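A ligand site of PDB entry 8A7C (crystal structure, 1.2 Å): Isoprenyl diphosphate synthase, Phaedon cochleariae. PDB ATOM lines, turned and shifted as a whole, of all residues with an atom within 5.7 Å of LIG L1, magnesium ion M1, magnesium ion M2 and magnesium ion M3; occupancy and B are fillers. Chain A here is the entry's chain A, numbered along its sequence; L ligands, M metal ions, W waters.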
ATOM      1  N   LEU A  92      10.363   5.370 -11.211  1.00  0.00           N
ATOM      2  CA  LEU A  92       8.934   5.209 -10.947  1.00  0.00           C
ATOM      3  C   LEU A  92       8.220   6.559 -11.010  1.00  0.00           C
ATOM      4  O   LEU A  92       7.108   6.641 -11.521  1.00  0.00           O
ATOM      5  CB  LEU A  92       8.739   4.525  -9.594  1.00  0.00           C
ATOM      6  CG  LEU A  92       9.174   3.064  -9.583  1.00  0.00           C
ATOM      7  CD1 LEU A  92       9.266   2.544  -8.148  1.00  0.00           C
ATOM      8  CD2 LEU A  92       8.265   2.198 -10.429  1.00  0.00           C
ATOM      9  N   LEU A  93       8.828   7.603 -10.457  1.00  0.00           N
ATOM     10  CA  LEU A  93       8.136   8.912 -10.411  1.00  0.00           C
ATOM     11  C   LEU A  93       8.016   9.534 -11.815  1.00  0.00           C
ATOM     12  O   LEU A  93       6.989  10.182 -12.130  1.00  0.00           O
ATOM     13  CB  LEU A  93       8.776   9.876  -9.437  1.00  0.00           C
ATOM     14  CG  LEU A  93       8.869   9.385  -7.973  1.00  0.00           C
ATOM     15  CD1 LEU A  93       9.400  10.514  -7.085  1.00  0.00           C
ATOM     16  CD2 LEU A  93       7.534   8.885  -7.448  1.00  0.00           C
ATOM     17  N   ASP A  96       5.145   7.673 -13.277  1.00  0.00           N
ATOM     18  CA  ASP A  96       3.938   7.921 -12.521  1.00  0.00           C
ATOM     19  C   ASP A  96       3.361   9.284 -12.869  1.00  0.00           C
ATOM     20  O   ASP A  96       2.131   9.420 -12.990  1.00  0.00           O
ATOM     21  CB  ASP A  96       4.238   7.779 -11.031  1.00  0.00           C
ATOM     22  CG  ASP A  96       3.005   8.020 -10.207  1.00  0.00           C
ATOM     23  OD1 ASP A  96       2.207   7.059 -10.065  1.00  0.00           O
ATOM     24  OD2 ASP A  96       2.862   9.153  -9.698  1.00  0.00           O
ATOM     25  N   ASP A  97       4.226  10.296 -12.985  1.00  0.00           N
ATOM     26  CA  ASP A  97       3.732  11.642 -13.325  1.00  0.00           C
ATOM     27  C   ASP A  97       3.102  11.709 -14.729  1.00  0.00           C
ATOM     28  O   ASP A  97       2.097  12.410 -14.904  1.00  0.00           O
ATOM     29  CB  ASP A  97       4.860  12.663 -13.156  1.00  0.00           C
ATOM     30  CG  ASP A  97       5.207  12.901 -11.683  1.00  0.00           C
ATOM     31  OD1 ASP A  97       4.289  12.734 -10.843  1.00  0.00           O
ATOM     32  OD2 ASP A  97       6.331  13.377 -11.418  1.00  0.00           O
ATOM     33  N   ASP A 100      -0.340   9.962 -14.265  1.00  0.00           N
ATOM     34  CA  ASP A 100      -1.269  10.675 -13.374  1.00  0.00           C
ATOM     35  C   ASP A 100      -1.529  12.090 -13.907  1.00  0.00           C
ATOM     36  O   ASP A 100      -2.304  12.827 -13.271  1.00  0.00           O
ATOM     37  CB  ASP A 100      -0.741  10.664 -11.937  1.00  0.00           C
ATOM     38  CG  ASP A 100      -0.708   9.263 -11.369  1.00  0.00           C
ATOM     39  OD1 ASP A 100      -1.367   8.382 -11.960  1.00  0.00           O
ATOM     40  OD2 ASP A 100      -0.040   9.015 -10.281  1.00  0.00           O
ATOM     41  N   SER A 102       0.304  14.690 -13.914  1.00  0.00           N
ATOM     42  CA  SER A 102       0.695  15.626 -12.844  1.00  0.00           C
ATOM     43  C   SER A 102       1.398  16.871 -13.393  1.00  0.00           C
ATOM     44  O   SER A 102       1.882  16.889 -14.510  1.00  0.00           O
ATOM     45  CB  SER A 102       1.526  14.857 -11.821  1.00  0.00           C
ATOM     46  OG  SER A 102       0.733  13.901 -11.124  1.00  0.00           O
ATOM     47  N   ARG A 105       6.607  18.039  -9.520  1.00  0.00           N
ATOM     48  CA  ARG A 105       7.272  16.984  -8.751  1.00  0.00           C
ATOM     49  C   ARG A 105       8.487  17.610  -8.081  1.00  0.00           C
ATOM     50  O   ARG A 105       9.286  18.233  -8.775  1.00  0.00           O
ATOM     51  CB  ARG A 105       7.690  15.847  -9.674  1.00  0.00           C
ATOM     52  CG  ARG A 105       8.567  14.798  -9.009  1.00  0.00           C
ATOM     53  CD  ARG A 105       7.876  13.959  -7.936  1.00  0.00           C
ATOM     54  NE  ARG A 105       6.844  13.118  -8.502  1.00  0.00           N
ATOM     55  CZ  ARG A 105       6.028  12.353  -7.772  1.00  0.00           C
ATOM     56  NH1 ARG A 105       6.182  12.276  -6.457  1.00  0.00           N
ATOM     57  NH2 ARG A 105       5.126  11.592  -8.373  1.00  0.00           N
ATOM     58  N   THR A 160       6.040  -4.002  -8.005  1.00  0.00           N
ATOM     59  CA  THR A 160       5.680  -2.566  -8.095  1.00  0.00           C
ATOM     60  C   THR A 160       4.841  -2.331  -9.351  1.00  0.00           C
ATOM     61  O   THR A 160       3.839  -1.604  -9.312  1.00  0.00           O
ATOM     62  CB  THR A 160       6.917  -1.679  -8.013  1.00  0.00           C
ATOM     63  OG1 THR A 160       7.663  -1.977  -6.824  1.00  0.00           O
ATOM     64  CG2 THR A 160       6.561  -0.222  -7.981  1.00  0.00           C
ATOM     65  N   GLN A 164       1.105  -0.697  -9.574  1.00  0.00           N
ATOM     66  CA  GLN A 164       0.812   0.471 -10.444  1.00  0.00           C
ATOM     67  C   GLN A 164      -0.359   0.106 -11.361  1.00  0.00           C
ATOM     68  O   GLN A 164      -1.175   0.974 -11.670  1.00  0.00           O
ATOM     69  CB  GLN A 164       2.074   0.843 -11.194  1.00  0.00           C
ATOM     70  CG  GLN A 164       1.994   2.156 -11.897  1.00  0.00           C
ATOM     71  CD  GLN A 164       2.107   3.352 -10.969  1.00  0.00           C
ATOM     72  OE1 GLN A 164       2.073   3.242  -9.672  1.00  0.00           O
ATOM     73  NE2 GLN A 164       2.267   4.486 -11.652  1.00  0.00           N
ATOM     74  N   ASP A 167      -3.621   0.099  -9.241  1.00  0.00           N
ATOM     75  CA  ASP A 167      -3.897   1.519  -8.995  1.00  0.00           C
ATOM     76  C   ASP A 167      -4.620   2.170 -10.208  1.00  0.00           C
ATOM     77  O   ASP A 167      -5.567   2.965 -10.044  1.00  0.00           O
ATOM     78  CB  ASP A 167      -2.602   2.234  -8.666  1.00  0.00           C
ATOM     79  CG  ASP A 167      -2.730   3.699  -8.385  1.00  0.00           C
ATOM     80  OD1 ASP A 167      -2.855   4.070  -7.184  1.00  0.00           O
ATOM     81  OD2 ASP A 167      -2.727   4.485  -9.348  1.00  0.00           O
ATOM     82  N   LYS A 193       2.154  -1.290  -4.848  1.00  0.00           N
ATOM     83  CA  LYS A 193       2.670  -0.084  -5.542  1.00  0.00           C
ATOM     84  C   LYS A 193       3.653   0.691  -4.707  1.00  0.00           C
ATOM     85  O   LYS A 193       4.373   1.541  -5.277  1.00  0.00           O
ATOM     86  CB  LYS A 193       1.545   0.850  -6.050  1.00  0.00           C
ATOM     87  CG  LYS A 193       0.935   1.739  -4.989  1.00  0.00           C
ATOM     88  CD  LYS A 193       0.127   2.874  -5.540  1.00  0.00           C
ATOM     89  CE  LYS A 193      -0.525   3.746  -4.475  1.00  0.00           C
ATOM     90  NZ  LYS A 193      -1.239   4.895  -5.046  1.00  0.00           N
ATOM     91  N   THR A 194       3.688   0.472  -3.400  1.00  0.00           N
ATOM     92  CA  THR A 194       4.499   1.315  -2.488  1.00  0.00           C
ATOM     93  C   THR A 194       5.330   0.474  -1.490  1.00  0.00           C
ATOM     94  O   THR A 194       6.513   0.755  -1.331  1.00  0.00           O
ATOM     95  CB  THR A 194       3.630   2.327  -1.749  1.00  0.00           C
ATOM     96  OG1 THR A 194       3.269   3.294  -2.753  1.00  0.00           O
ATOM     97  CG2 THR A 194       4.342   2.970  -0.579  1.00  0.00           C
ATOM     98  N   TYR A 197       8.843  -1.528  -2.456  1.00  0.00           N
ATOM     99  CA  TYR A 197      10.045  -0.784  -2.874  1.00  0.00           C
ATOM    100  C   TYR A 197      10.445   0.272  -1.860  1.00  0.00           C
ATOM    101  O   TYR A 197      11.630   0.620  -1.821  1.00  0.00           O
ATOM    102  CB  TYR A 197       9.926  -0.227  -4.280  1.00  0.00           C
ATOM    103  CG  TYR A 197       9.329   1.157  -4.396  1.00  0.00           C
ATOM    104  CD1 TYR A 197      10.158   2.275  -4.419  1.00  0.00           C
ATOM    105  CD2 TYR A 197       7.960   1.421  -4.478  1.00  0.00           C
ATOM    106  CE1 TYR A 197       9.698   3.574  -4.579  1.00  0.00           C
ATOM    107  CE2 TYR A 197       7.477   2.722  -4.599  1.00  0.00           C
ATOM    108  CZ  TYR A 197       8.343   3.790  -4.638  1.00  0.00           C
ATOM    109  OH  TYR A 197       7.822   5.040  -4.796  1.00  0.00           O
ATOM    110  N   GLN A 233       1.534   5.352   2.786  1.00  0.00           N
ATOM    111  CA  GLN A 233       0.712   5.670   1.585  1.00  0.00           C
ATOM    112  C   GLN A 233      -0.567   6.394   1.997  1.00  0.00           C
ATOM    113  O   GLN A 233      -1.048   7.257   1.236  1.00  0.00           O
ATOM    114  CB  GLN A 233       0.437   4.415   0.759  1.00  0.00           C
ATOM    115  CG  GLN A 233      -0.235   4.754  -0.576  1.00  0.00           C
ATOM    116  CD  GLN A 233       0.632   5.599  -1.476  1.00  0.00           C
ATOM    117  OE1 GLN A 233       1.804   5.326  -1.690  1.00  0.00           O
ATOM    118  NE2 GLN A 233       0.001   6.636  -2.036  1.00  0.00           N
ATOM    119  N   ASP A 236       0.426   9.825   2.217  1.00  0.00           N
ATOM    120  CA  ASP A 236       0.589  10.407   0.872  1.00  0.00           C
ATOM    121  C   ASP A 236      -0.785  10.831   0.292  1.00  0.00           C
ATOM    122  O   ASP A 236      -0.906  11.880  -0.344  1.00  0.00           O
ATOM    123  CB  ASP A 236       1.257   9.428  -0.079  1.00  0.00           C
ATOM    124  CG  ASP A 236       1.516  10.009  -1.444  1.00  0.00           C
ATOM    125  OD1 ASP A 236       2.343  10.954  -1.493  1.00  0.00           O
ATOM    126  OD2 ASP A 236       0.867   9.529  -2.429  1.00  0.00           O
ATOM    127  N   ASP A 237      -1.768   9.966   0.484  1.00  0.00           N
ATOM    128  CA  ASP A 237      -3.128  10.225  -0.042  1.00  0.00           C
ATOM    129  C   ASP A 237      -3.731  11.441   0.652  1.00  0.00           C
ATOM    130  O   ASP A 237      -4.399  12.283  -0.012  1.00  0.00           O
ATOM    131  CB  ASP A 237      -4.003   9.000   0.149  1.00  0.00           C
ATOM    132  CG  ASP A 237      -3.621   7.781  -0.673  1.00  0.00           C
ATOM    133  OD1 ASP A 237      -2.692   7.871  -1.486  1.00  0.00           O
ATOM    134  OD2 ASP A 237      -4.296   6.743  -0.430  1.00  0.00           O
ATOM    135  N   ASP A 240      -2.258  14.526  -0.943  1.00  0.00           N
ATOM    136  CA  ASP A 240      -2.734  14.844  -2.325  1.00  0.00           C
ATOM    137  C   ASP A 240      -3.853  15.885  -2.258  1.00  0.00           C
ATOM    138  O   ASP A 240      -3.852  16.813  -3.101  1.00  0.00           O
ATOM    139  CB  ASP A 240      -3.219  13.569  -3.013  1.00  0.00           C
ATOM    140  CG  ASP A 240      -3.533  13.787  -4.479  1.00  0.00           C
ATOM    141  OD1 ASP A 240      -2.621  13.656  -5.303  1.00  0.00           O
ATOM    142  OD2 ASP A 240      -4.677  14.111  -4.771  1.00  0.00           O
ATOM    143  N   LYS A 250       4.392  18.936  -4.931  1.00  0.00           N
ATOM    144  CA  LYS A 250       3.564  18.308  -5.959  1.00  0.00           C
ATOM    145  C   LYS A 250       2.110  18.744  -5.779  1.00  0.00           C
ATOM    146  O   LYS A 250       1.599  18.872  -4.688  1.00  0.00           O
ATOM    147  CB  LYS A 250       3.719  16.785  -5.946  1.00  0.00           C
ATOM    148  CG  LYS A 250       3.314  16.064  -4.682  1.00  0.00           C
ATOM    149  CD  LYS A 250       3.840  14.615  -4.604  1.00  0.00           C
ATOM    150  CE  LYS A 250       3.163  13.844  -3.506  1.00  0.00           C
ATOM    151  NZ  LYS A 250       3.694  12.488  -3.350  1.00  0.00           N
ATOM    152  N   THR A 253      -3.662  15.136  -7.760  1.00  0.00           N
ATOM    153  CA  THR A 253      -4.481  14.715  -8.939  1.00  0.00           C
ATOM    154  C   THR A 253      -5.443  13.577  -8.609  1.00  0.00           C
ATOM    155  O   THR A 253      -6.072  13.071  -9.519  1.00  0.00           O
ATOM    156  CB  THR A 253      -3.578  14.277 -10.101  1.00  0.00           C
ATOM    157  OG1 THR A 253      -2.726  13.226  -9.657  1.00  0.00           O
ATOM    158  CG2 THR A 253      -2.762  15.409 -10.649  1.00  0.00           C
ATOM    159  N   ASP A 254      -5.467  13.050  -7.369  1.00  0.00           N
ATOM    160  CA  ASP A 254      -6.208  11.803  -7.169  1.00  0.00           C
ATOM    161  C   ASP A 254      -7.708  11.919  -7.460  1.00  0.00           C
ATOM    162  O   ASP A 254      -8.300  10.972  -7.992  1.00  0.00           O
ATOM    163  CB  ASP A 254      -6.021  11.253  -5.732  1.00  0.00           C
ATOM    164  CG  ASP A 254      -4.628  10.730  -5.414  1.00  0.00           C
ATOM    165  OD1 ASP A 254      -3.862  10.409  -6.375  1.00  0.00           O
ATOM    166  OD2 ASP A 254      -4.329  10.614  -4.189  1.00  0.00           O
ATOM    167  N   LYS A 259      -8.986   8.075  -8.391  1.00  0.00           N
ATOM    168  CA  LYS A 259      -8.203   7.033  -7.700  1.00  0.00           C
ATOM    169  C   LYS A 259      -8.937   6.465  -6.488  1.00  0.00           C
ATOM    170  O   LYS A 259      -9.655   7.155  -5.765  1.00  0.00           O
ATOM    171  CB  LYS A 259      -6.905   7.652  -7.252  1.00  0.00           C
ATOM    172  CG  LYS A 259      -5.932   8.018  -8.381  1.00  0.00           C
ATOM    173  CD  LYS A 259      -5.330   6.780  -9.046  1.00  0.00           C
ATOM    174  CE  LYS A 259      -4.889   6.925 -10.474  1.00  0.00           C
ATOM    175  NZ  LYS A 259      -3.883   7.989 -10.527  1.00  0.00           N
HETATM  176  O1  LIG L   1       0.751   6.447  -6.039  1.00  0.00           O
HETATM  177  P1  LIG L   1       0.833   7.932  -6.260  1.00  0.00           P
HETATM  178  O2  LIG L   1       0.720   8.311  -7.773  1.00  0.00           O
HETATM  179  O3  LIG L   1      -0.151   8.705  -5.375  1.00  0.00           O
HETATM  180  C1  LIG L   1       2.507   8.524  -5.720  1.00  0.00           C
HETATM  181  P2  LIG L   1       2.656  10.363  -5.884  1.00  0.00           P
HETATM  182  O4  LIG L   1       1.653  10.943  -4.929  1.00  0.00           O
HETATM  183  O5  LIG L   1       2.348  10.742  -7.323  1.00  0.00           O
HETATM  184  O6  LIG L   1       4.087  10.716  -5.497  1.00  0.00           O
HETATM  185  O7  LIG L   1       2.662   8.200  -4.325  1.00  0.00           O
HETATM  186  C2  LIG L   1       3.628   7.837  -6.501  1.00  0.00           C
HETATM  187  N1  LIG L   1       3.672   6.373  -6.322  1.00  0.00           N
HETATM  188  C3  LIG L   1       3.695   5.662  -5.166  1.00  0.00           C
HETATM  189  N2  LIG L   1       3.764   4.386  -5.415  1.00  0.00           N
HETATM  190  C4  LIG L   1       3.780   4.225  -6.759  1.00  0.00           C
HETATM  191  C5  LIG L   1       3.747   5.460  -7.348  1.00  0.00           C
HETATM  192  C1  LG2 L   2       6.614   9.471  -3.105  1.00  0.00           C
HETATM  193  O1  LG2 L   2       7.676   9.168  -2.179  1.00  0.00           O
HETATM  194  C2  LG2 L   2       5.945   8.217  -3.584  1.00  0.00           C
HETATM  195  C3  LG2 L   2       5.346   7.362  -2.491  1.00  0.00           C
HETATM  196  C4  LG2 L   2       5.556   6.060  -2.448  1.00  0.00           C
HETATM  197  C5  LG2 L   2       4.404   8.064  -1.549  1.00  0.00           C
HETATM  198  P1  LG2 L   2       8.305  10.283  -1.260  1.00  0.00           P
HETATM  199  O2  LG2 L   2       7.240  11.108  -0.659  1.00  0.00           O
HETATM  200  O3  LG2 L   2       9.278   9.576  -0.370  1.00  0.00           O
HETATM  201  O4  LG2 L   2       9.063  11.193  -2.318  1.00  0.00           O
HETATM  202  P2  LG2 L   2      10.582  11.758  -2.547  1.00  0.00           P
HETATM  203  O5  LG2 L   2      10.394  12.972  -3.481  1.00  0.00           O
HETATM  204  O6  LG2 L   2      11.075  12.168  -1.181  1.00  0.00           O
HETATM  205  O7  LG2 L   2      11.361  10.660  -3.174  1.00  0.00           O
HETATM  206 MG    MG M   1       1.219  10.042  -8.876  1.00  0.00          MG
HETATM  207 MG    MG M   2       0.227   7.109  -9.395  1.00  0.00          MG
HETATM  208 MG    MG M   3      -0.090  10.370  -4.141  1.00  0.00          MG
HETATM  209  O   HOH W   1      -2.599   7.963  -6.276  1.00  0.00           O
HETATM  210  O   HOH W   2      -1.317  11.357  -5.621  1.00  0.00           O
HETATM  211  O   HOH W   3       1.753  13.506  -7.266  1.00  0.00           O
HETATM  212  O   HOH W   4       1.820  11.645 -10.072  1.00  0.00           O
HETATM  213  O   HOH W   5      -0.249   6.160 -11.161  1.00  0.00           O
HETATM  214  O   HOH W   6      -1.790   6.992  -8.749  1.00  0.00           O
HETATM  215  O   HOH W   7       0.537   5.320  -8.425  1.00  0.00           O
HETATM  216  O   HOH W   8      -0.491  11.080  -8.284  1.00  0.00           O
HETATM  217  O   HOH W   9      -1.899   9.824  -3.279  1.00  0.00           O
HETATM  218  O   HOH W  10      -0.153  12.190  -3.058  1.00  0.00           O
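Within 4 Å of magnesium ion M1: Asp 96 and Asp 100.
Residues that only touch magnesium ion M2: Asp 167 (3.95 Å).
Of the 21 residues printed, 3 come within 4 Å of magnesium ion M2.
Along chain A the residues within 4 Å of magnesium ion M2 span positions 96 to 167.
O4 of LIG L1 is bound to magnesium ion M3, at 2.0 Å.
Magnesium ion M3 is bound by an oxygen (O3) of LIG L1, 2.1 Å away.
Magnesium ion M3 is bound by water W9, 2.1 Å away.
Water W10 binds magnesium ion M3, 2.1 Å away.
OD2 of Asp 236 binds magnesium ion M3 (2.1 Å).
Water W2 is bound to magnesium ion M3.
Magnesium ion M1 is bound by the side-chain carboxylate (OD2) of Asp 96 (2.0 Å), an oxygen (O5) of LIG L1 (2.0 Å), water W8 (2.1 Å), water W4 (2.1 Å), an oxygen (O2) of LIG L1 (2.1 Å) and the side-chain carboxylate (OD2) of Asp 100 (2.1 Å).
OD2 of Asp 96 sits close to NH2 of Arg 105.
The side-chain carboxylate of Asp 236 sits close to the side-chain amide nitrogen of Gln 233 (3.0 Å).
The side-chain carboxylate (OD1) of Asp 100 lies within salt-bridge range of the side-chain amino group (NZ) of Lys 259, 2.9 Å away.
The side-chain carboxylate (OD1) of Asp 97 lies within salt-bridge range of the guanidinium group (NH2) of Arg 105, at 2.8 Å.
The side-chain amide nitrogen (NE2) of Gln 233 is in hydrogen-bond range of the side-chain carboxylate (OD1) of Asp 237.
The side-chain amide oxygen of Gln 233 is in hydrogen-bond range of the side-chain hydroxyl of Thr 194, at 2.7 Å.
The side-chain amino group (NZ) of Lys 259 lies within salt-bridge range of the side-chain carboxylate (OD2) of Asp 167.
OD1 of Asp 236 is in salt-bridge range of NZ of Lys 250 (2.8 Å).
The nearest printed residue that does not touch magnesium ion M3 is Asp 254 (4.2 Å).
NH1 of Arg 105 lies within salt-bridge range of O6 of LIG L1, 2.8 Å away.
O1 of LIG L1 lies within salt-bridge range of NZ of Lys 193 (2.7 Å).
OG1 of Thr 194 sits at hydrogen-bond distance from N2 of LIG L1, at 2.9 Å.
An oxygen (O6) of LIG L1 is in salt-bridge range of the side-chain amino group (NZ) of Lys 250, at 2.8 Å.
Magnesium ion M2 is bound by water W7, water W5, O2 of LIG L1, OD1 of Asp 96, OD2 of Asp 100 and water W6.
Water W4 bridges OG of Ser 102 (2.7 Å) and OD1 of Asp 97 (2.8 Å).
Water W7 lies within hydrogen-bond range of an oxygen (O1) of LIG L1 (2.6 Å), the side-chain amide oxygen (OE1) of Gln 164 (2.9 Å) and the side-chain carboxylate (OD2) of Asp 167 (3.5 Å).
Water W5 lies within hydrogen-bond range of the side-chain carboxylate of Asp 100 (2.6 Å), the side-chain amide nitrogen of Gln 164 (3.1 Å) and the side-chain carboxylate of Asp 167 (3.5 Å).
Water W6 bridges the side-chain carboxylate of Asp 167 (2.7 Å) and the side-chain amino group of Lys 259 (2.9 Å).
Water W2 bridges the side-chain carboxylate of Asp 240 and the side-chain carboxylate of Asp 254.
Water W9 lies within hydrogen-bond range of OD2 of Asp 254 and OD1 of Asp 237.
Merely in contact with LIG L1: Gln 164 (3.5 Å) and Gln 233 (3.8 Å).
The nearest printed residue that does not touch LIG L1 is Tyr 197 (4.1 Å).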
